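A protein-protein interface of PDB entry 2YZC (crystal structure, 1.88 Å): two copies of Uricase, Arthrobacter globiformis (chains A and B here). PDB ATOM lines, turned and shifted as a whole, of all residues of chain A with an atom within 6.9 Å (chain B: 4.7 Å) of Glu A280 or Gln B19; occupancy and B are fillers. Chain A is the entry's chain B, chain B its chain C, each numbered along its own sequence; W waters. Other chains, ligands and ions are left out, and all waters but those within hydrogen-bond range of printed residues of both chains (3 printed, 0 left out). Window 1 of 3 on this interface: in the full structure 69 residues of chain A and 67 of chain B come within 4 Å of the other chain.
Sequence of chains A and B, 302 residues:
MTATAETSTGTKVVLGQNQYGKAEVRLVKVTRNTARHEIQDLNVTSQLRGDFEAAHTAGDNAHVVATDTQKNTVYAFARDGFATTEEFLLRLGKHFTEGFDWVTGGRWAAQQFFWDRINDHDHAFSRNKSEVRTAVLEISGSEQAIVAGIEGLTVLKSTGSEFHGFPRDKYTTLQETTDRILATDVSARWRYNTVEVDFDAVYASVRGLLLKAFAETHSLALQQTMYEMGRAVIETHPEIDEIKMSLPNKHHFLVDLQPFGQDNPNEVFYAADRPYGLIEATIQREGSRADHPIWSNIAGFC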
ATOM      1  N   GLN A 223       4.998 -15.574 -30.252  1.00  0.00           N
ATOM      2  CA  GLN A 223       6.051 -15.891 -31.217  1.00  0.00           C
ATOM      3  C   GLN A 223       5.996 -14.973 -32.436  1.00  0.00           C
ATOM      4  O   GLN A 223       7.035 -14.573 -32.972  1.00  0.00           O
ATOM      5  CB  GLN A 223       5.946 -17.355 -31.677  1.00  0.00           C
ATOM      6  CG  GLN A 223       6.326 -18.383 -30.614  1.00  0.00           C
ATOM      7  CD  GLN A 223       5.147 -18.841 -29.783  1.00  0.00           C
ATOM      8  OE1 GLN A 223       4.236 -18.064 -29.492  1.00  0.00           O
ATOM      9  NE2 GLN A 223       5.163 -20.108 -29.381  1.00  0.00           N
ATOM     10  N   MET A 226       7.082 -11.355 -31.458  1.00  0.00           N
ATOM     11  CA  MET A 226       8.534 -11.327 -31.349  1.00  0.00           C
ATOM     12  C   MET A 226       9.183 -11.350 -32.734  1.00  0.00           C
ATOM     13  O   MET A 226      10.168 -10.654 -32.987  1.00  0.00           O
ATOM     14  CB  MET A 226       9.020 -12.523 -30.528  1.00  0.00           C
ATOM     15  CG  MET A 226      10.537 -12.652 -30.436  1.00  0.00           C
ATOM     16  SD  MET A 226      11.034 -13.973 -29.315  1.00  0.00           S
ATOM     17  CE  MET A 226      10.357 -15.392 -30.202  1.00  0.00           C
ATOM     18  N   LYS A 244      18.501 -11.361 -30.787  1.00  0.00           N
ATOM     19  CA  LYS A 244      17.940 -12.437 -29.993  1.00  0.00           C
ATOM     20  C   LYS A 244      17.033 -11.840 -28.937  1.00  0.00           C
ATOM     21  O   LYS A 244      17.388 -10.858 -28.288  1.00  0.00           O
ATOM     22  CB  LYS A 244      19.056 -13.238 -29.315  1.00  0.00           C
ATOM     23  CG  LYS A 244      19.957 -13.975 -30.293  1.00  0.00           C
ATOM     24  CD  LYS A 244      20.904 -14.926 -29.581  1.00  0.00           C
ATOM     25  CE  LYS A 244      21.693 -15.749 -30.595  1.00  0.00           C
ATOM     26  NZ  LYS A 244      22.537 -16.774 -29.930  1.00  0.00           N
ATOM     27  N   MET A 245      15.859 -12.433 -28.768  1.00  0.00           N
ATOM     28  CA  MET A 245      14.922 -11.950 -27.770  1.00  0.00           C
ATOM     29  C   MET A 245      14.438 -13.079 -26.876  1.00  0.00           C
ATOM     30  O   MET A 245      14.328 -14.233 -27.307  1.00  0.00           O
ATOM     31  CB  MET A 245      13.737 -11.279 -28.451  1.00  0.00           C
ATOM     32  CG  MET A 245      14.109  -9.999 -29.167  1.00  0.00           C
ATOM     33  SD  MET A 245      12.781  -9.432 -30.219  1.00  0.00           S
ATOM     34  CE  MET A 245      13.064 -10.428 -31.657  1.00  0.00           C
ATOM     35  N   SER A 246      14.165 -12.730 -25.624  1.00  0.00           N
ATOM     36  CA  SER A 246      13.674 -13.671 -24.633  1.00  0.00           C
ATOM     37  C   SER A 246      12.500 -12.945 -24.007  1.00  0.00           C
ATOM     38  O   SER A 246      12.686 -11.992 -23.248  1.00  0.00           O
ATOM     39  CB  SER A 246      14.748 -13.949 -23.582  1.00  0.00           C
ATOM     40  OG  SER A 246      14.249 -14.808 -22.570  1.00  0.00           O
ATOM     41  N   LEU A 247      11.294 -13.394 -24.334  1.00  0.00           N
ATOM     42  CA  LEU A 247      10.090 -12.748 -23.844  1.00  0.00           C
ATOM     43  C   LEU A 247       9.190 -13.627 -22.992  1.00  0.00           C
ATOM     44  O   LEU A 247       8.668 -14.641 -23.453  1.00  0.00           O
ATOM     45  CB  LEU A 247       9.280 -12.212 -25.029  1.00  0.00           C
ATOM     46  CG  LEU A 247       9.992 -11.262 -26.001  1.00  0.00           C
ATOM     47  CD1 LEU A 247       9.055 -10.881 -27.132  1.00  0.00           C
ATOM     48  CD2 LEU A 247      10.457 -10.021 -25.256  1.00  0.00           C
ATOM     49  N   LEU A 278       7.648 -18.689 -21.618  1.00  0.00           N
ATOM     50  CA  LEU A 278       8.937 -18.105 -21.979  1.00  0.00           C
ATOM     51  C   LEU A 278       9.186 -18.422 -23.449  1.00  0.00           C
ATOM     52  O   LEU A 278       9.451 -19.565 -23.812  1.00  0.00           O
ATOM     53  CB  LEU A 278      10.060 -18.679 -21.108  1.00  0.00           C
ATOM     54  CG  LEU A 278      11.448 -18.060 -21.310  1.00  0.00           C
ATOM     55  CD1 LEU A 278      11.380 -16.548 -21.138  1.00  0.00           C
ATOM     56  CD2 LEU A 278      12.428 -18.664 -20.318  1.00  0.00           C
ATOM     57  N   ILE A 279       9.076 -17.393 -24.283  1.00  0.00           N
ATOM     58  CA  ILE A 279       9.249 -17.511 -25.731  1.00  0.00           C
ATOM     59  C   ILE A 279      10.566 -16.860 -26.126  1.00  0.00           C
ATOM     60  O   ILE A 279      10.781 -15.688 -25.838  1.00  0.00           O
ATOM     61  CB  ILE A 279       8.075 -16.803 -26.466  1.00  0.00           C
ATOM     62  CG1 ILE A 279       6.843 -17.708 -26.494  1.00  0.00           C
ATOM     63  CG2 ILE A 279       8.471 -16.451 -27.883  1.00  0.00           C
ATOM     64  CD1 ILE A 279       6.326 -18.118 -25.129  1.00  0.00           C
ATOM     65  N   GLU A 280      11.440 -17.613 -26.792  1.00  0.00           N
ATOM     66  CA  GLU A 280      12.743 -17.084 -27.184  1.00  0.00           C
ATOM     67  C   GLU A 280      13.078 -17.401 -28.639  1.00  0.00           C
ATOM     68  O   GLU A 280      12.709 -18.456 -29.156  1.00  0.00           O
ATOM     69  CB  GLU A 280      13.825 -17.662 -26.266  1.00  0.00           C
ATOM     70  CG  GLU A 280      13.394 -17.728 -24.797  1.00  0.00           C
ATOM     71  CD  GLU A 280      14.516 -18.131 -23.859  1.00  0.00           C
ATOM     72  OE1 GLU A 280      15.280 -17.240 -23.426  1.00  0.00           O
ATOM     73  OE2 GLU A 280      14.635 -19.339 -23.557  1.00  0.00           O
ATOM     74  N   ALA A 281      13.781 -16.485 -29.299  1.00  0.00           N
ATOM     75  CA  ALA A 281      14.146 -16.706 -30.691  1.00  0.00           C
ATOM     76  C   ALA A 281      15.210 -15.757 -31.192  1.00  0.00           C
ATOM     77  O   ALA A 281      15.419 -14.674 -30.643  1.00  0.00           O
ATOM     78  CB  ALA A 281      12.918 -16.597 -31.584  1.00  0.00           C
ATOM     79  N   THR A 282      15.874 -16.190 -32.256  1.00  0.00           N
ATOM     80  CA  THR A 282      16.908 -15.414 -32.906  1.00  0.00           C
ATOM     81  C   THR A 282      16.361 -15.060 -34.279  1.00  0.00           C
ATOM     82  O   THR A 282      15.877 -15.931 -35.003  1.00  0.00           O
ATOM     83  CB  THR A 282      18.191 -16.232 -33.124  1.00  0.00           C
ATOM     84  OG1 THR A 282      18.665 -16.741 -31.872  1.00  0.00           O
ATOM     85  CG2 THR A 282      19.265 -15.363 -33.767  1.00  0.00           C
ATOM     86  N   GLN B  17      17.575 -20.003 -34.423  1.00  0.00           N
ATOM     87  CA  GLN B  17      17.308 -20.885 -33.295  1.00  0.00           C
ATOM     88  C   GLN B  17      16.152 -20.288 -32.500  1.00  0.00           C
ATOM     89  O   GLN B  17      16.034 -19.067 -32.389  1.00  0.00           O
ATOM     90  CB  GLN B  17      18.545 -20.986 -32.402  1.00  0.00           C
ATOM     91  CG  GLN B  17      19.784 -21.506 -33.113  1.00  0.00           C
ATOM     92  CD  GLN B  17      21.021 -21.434 -32.237  1.00  0.00           C
ATOM     93  OE1 GLN B  17      21.409 -20.356 -31.778  1.00  0.00           O
ATOM     94  NE2 GLN B  17      21.648 -22.583 -32.000  1.00  0.00           N
ATOM     95  N   ASN B  18      15.290 -21.146 -31.966  1.00  0.00           N
ATOM     96  CA  ASN B  18      14.159 -20.674 -31.180  1.00  0.00           C
ATOM     97  C   ASN B  18      13.632 -21.790 -30.291  1.00  0.00           C
ATOM     98  O   ASN B  18      13.833 -22.971 -30.576  1.00  0.00           O
ATOM     99  CB  ASN B  18      13.048 -20.148 -32.102  1.00  0.00           C
ATOM    100  CG  ASN B  18      12.434 -21.235 -32.969  1.00  0.00           C
ATOM    101  OD1 ASN B  18      11.543 -21.963 -32.535  1.00  0.00           O
ATOM    102  ND2 ASN B  18      12.919 -21.352 -34.200  1.00  0.00           N
ATOM    103  N   GLN B  19      12.977 -21.407 -29.202  1.00  0.00           N
ATOM    104  CA  GLN B  19      12.421 -22.374 -28.262  1.00  0.00           C
ATOM    105  C   GLN B  19      11.377 -21.676 -27.412  1.00  0.00           C
ATOM    106  O   GLN B  19      11.424 -20.457 -27.252  1.00  0.00           O
ATOM    107  CB  GLN B  19      13.522 -22.934 -27.358  1.00  0.00           C
ATOM    108  CG  GLN B  19      14.263 -21.871 -26.547  1.00  0.00           C
ATOM    109  CD  GLN B  19      15.373 -22.458 -25.691  1.00  0.00           C
ATOM    110  OE1 GLN B  19      15.944 -23.493 -26.025  1.00  0.00           O
ATOM    111  NE2 GLN B  19      15.699 -21.785 -24.592  1.00  0.00           N
ATOM    112  N   TYR B  20      10.436 -22.441 -26.869  1.00  0.00           N
ATOM    113  CA  TYR B  20       9.396 -21.848 -26.034  1.00  0.00           C
ATOM    114  C   TYR B  20       8.785 -22.887 -25.102  1.00  0.00           C
ATOM    115  O   TYR B  20       8.844 -24.092 -25.361  1.00  0.00           O
ATOM    116  CB  TYR B  20       8.284 -21.257 -26.903  1.00  0.00           C
ATOM    117  CG  TYR B  20       7.283 -22.306 -27.331  1.00  0.00           C
ATOM    118  CD1 TYR B  20       7.623 -23.276 -28.270  1.00  0.00           C
ATOM    119  CD2 TYR B  20       6.037 -22.393 -26.715  1.00  0.00           C
ATOM    120  CE1 TYR B  20       6.753 -24.311 -28.576  1.00  0.00           C
ATOM    121  CE2 TYR B  20       5.158 -23.424 -27.014  1.00  0.00           C
ATOM    122  CZ  TYR B  20       5.525 -24.382 -27.944  1.00  0.00           C
ATOM    123  OH  TYR B  20       4.673 -25.419 -28.234  1.00  0.00           O
ATOM    124  N   GLN B  47      10.899 -26.291 -22.252  1.00  0.00           N
ATOM    125  CA  GLN B  47      10.911 -25.561 -23.513  1.00  0.00           C
ATOM    126  C   GLN B  47      11.119 -26.535 -24.664  1.00  0.00           C
ATOM    127  O   GLN B  47      11.945 -27.447 -24.587  1.00  0.00           O
ATOM    128  CB  GLN B  47      11.985 -24.478 -23.509  1.00  0.00           C
ATOM    129  CG  GLN B  47      11.569 -23.244 -22.704  1.00  0.00           C
ATOM    130  CD  GLN B  47      12.614 -22.153 -22.730  1.00  0.00           C
ATOM    131  OE1 GLN B  47      12.318 -21.001 -23.040  1.00  0.00           O
ATOM    132  NE2 GLN B  47      13.843 -22.511 -22.407  1.00  0.00           N
ATOM    133  N   LEU B  48      10.350 -26.338 -25.728  1.00  0.00           N
ATOM    134  CA  LEU B  48      10.406 -27.221 -26.881  1.00  0.00           C
ATOM    135  C   LEU B  48      11.108 -26.591 -28.073  1.00  0.00           C
ATOM    136  O   LEU B  48      11.141 -25.372 -28.215  1.00  0.00           O
ATOM    137  CB  LEU B  48       8.983 -27.626 -27.284  1.00  0.00           C
ATOM    138  CG  LEU B  48       8.036 -28.043 -26.154  1.00  0.00           C
ATOM    139  CD1 LEU B  48       6.689 -28.441 -26.741  1.00  0.00           C
ATOM    140  CD2 LEU B  48       8.627 -29.192 -25.360  1.00  0.00           C
ATOM    141  N   ARG B  49      11.670 -27.446 -28.923  1.00  0.00           N
ATOM    142  CA  ARG B  49      12.363 -27.016 -30.130  1.00  0.00           C
ATOM    143  C   ARG B  49      11.871 -27.886 -31.279  1.00  0.00           C
ATOM    144  O   ARG B  49      11.514 -29.043 -31.075  1.00  0.00           O
ATOM    145  CB  ARG B  49      13.876 -27.182 -29.971  1.00  0.00           C
ATOM    146  CG  ARG B  49      14.488 -26.279 -28.912  1.00  0.00           C
ATOM    147  CD  ARG B  49      15.901 -26.721 -28.570  1.00  0.00           C
ATOM    148  NE  ARG B  49      16.498 -25.880 -27.536  1.00  0.00           N
ATOM    149  CZ  ARG B  49      17.661 -26.133 -26.948  1.00  0.00           C
ATOM    150  NH1 ARG B  49      18.354 -27.212 -27.284  1.00  0.00           N
ATOM    151  NH2 ARG B  49      18.136 -25.299 -26.036  1.00  0.00           N
ATOM    152  N   ARG B 107      14.657 -28.389 -24.058  1.00  0.00           N
ATOM    153  CA  ARG B 107      15.500 -28.189 -22.895  1.00  0.00           C
ATOM    154  C   ARG B 107      14.583 -28.213 -21.685  1.00  0.00           C
ATOM    155  O   ARG B 107      13.642 -27.425 -21.591  1.00  0.00           O
ATOM    156  CB  ARG B 107      16.213 -26.837 -22.996  1.00  0.00           C
ATOM    157  CG  ARG B 107      17.200 -26.546 -21.869  1.00  0.00           C
ATOM    158  CD  ARG B 107      17.703 -25.114 -21.959  1.00  0.00           C
ATOM    159  NE  ARG B 107      18.634 -24.772 -20.882  1.00  0.00           N
ATOM    160  CZ  ARG B 107      19.933 -25.070 -20.875  1.00  0.00           C
ATOM    161  NH1 ARG B 107      20.484 -25.724 -21.893  1.00  0.00           N
ATOM    162  NH2 ARG B 107      20.687 -24.713 -19.840  1.00  0.00           N
ATOM    163  N   ASN B 297      22.605 -23.141 -24.409  1.00  0.00           N
ATOM    164  CA  ASN B 297      21.283 -22.793 -23.891  1.00  0.00           C
ATOM    165  C   ASN B 297      20.449 -22.053 -24.936  1.00  0.00           C
ATOM    166  O   ASN B 297      19.279 -22.444 -25.131  1.00  0.00           O
ATOM    167  CB  ASN B 297      21.417 -21.942 -22.627  1.00  0.00           C
HETATM  168  O   HOH W   1       9.991 -18.720 -29.923  1.00  0.00           O
HETATM  169  O   HOH W   2      15.661 -20.894 -21.044  1.00  0.00           O
HETATM  170  O   HOH W   3      17.719 -17.824 -29.594  1.00  0.00           O
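O of Leu A278 sits close to OE1 of Gln B47 (3.3 Å). The side-chain amide nitrogen (NE2) of Gln B19 lies within hydrogen-bond range of the side-chain carboxylate (OE2) of Glu A280, 2.9 Å away. OE2 of Glu A280 sits close to OE1 of Gln B47, 2.9 Å away. The backbone NH (N) of Thr A282 is in hydrogen-bond range of the backbone carbonyl oxygen (O) of Gln B17 (2.9 Å).
N of Met A245 lies within hydrogen-bond range of O of Ala A281, 3.0 Å away. N of Leu A247 lies within hydrogen-bond range of O of Ile A279 (2.8 Å). The side-chain amide nitrogen of Gln B19 sits close to the side-chain amide nitrogen of Gln B47, at 3.0 Å. NH2 of Arg B49 sits at hydrogen-bond distance from OE1 of Gln B19 (2.8 Å). O of Tyr B20 lies within hydrogen-bond range of N of Leu B48, at 2.7 Å. O of Gln B47 is in hydrogen-bond range of N of Arg B107 (2.9 Å).
NE2 of Gln A223 touches CD2 of Tyr B20 (3.6 Å). O of Leu A278 touches CA of Tyr B20, 3.2 Å away. Gln B19 touches Ile A279. Tyr B20 touches Ile A279. Asn B18 touches Glu A280. Ala A281 touches Gln B17 (CA to O, 3.5 Å). Ala A281 touches Asn B18 (CB to CB, 3.6 Å).
Of chain B, only Asn B18 (3.3 Å), Gln B19 (2.9 Å) and Gln B47 (2.9 Å) come within 4 Å of Glu A280. Gln B19 touches just these residues of chain A: Ile A279 (3.9 Å) and Glu A280 (2.9 Å). Printed residues of chain B within 4 Å of Thr A282: Gln B17. Printed residues of chain A within 4 Å of Asn B18: Glu A280 (3.3 Å) and Ala A281 (3.6 Å). Of the printed residues of chain B, Ala A281 touches Gln B17 and Asn B18. Leu A247 touches none of the printed residues of chain B. The nearest residue of chain A that does not touch Gln B19 is Leu A278 (4.1 Å).
Of the 11 printed residues of chain A, 6 touch a printed residue of chain B. Hydrophobic or aromatic side chains of chain A within 4 Å of the printed part of chain B: Leu A278, Ile A279 and Ala A281. Of the 9 printed residues of chain B, 5 touch a printed residue of chain A. Hydrophobic or aromatic side chains of chain B within 4 Å of the printed part of chain A: Tyr B20. Among the printed residues, no Asp or Glu carboxylate lies within 4 Å of a Lys or Arg side-chain nitrogen of the other chain.
No position is printed for both chains. Of the 11 pairs that touch across the chains among the printed residues, none has its exchanged pair printed and touching as well.
Water W3 lies within hydrogen-bond range of the side-chain hydroxyl (OG1) of Thr A282 (2.7 Å) and the backbone carbonyl oxygen (O) of Gln B17 (3.5 Å). Water W2 lies within hydrogen-bond range of the side-chain amide nitrogen of Gln B47 and the side-chain carboxylate of Glu A280. Water W1 lies within hydrogen-bond range of the backbone carbonyl oxygen (O) of Glu A280 and the backbone carbonyl oxygen (O) of Gln B19.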
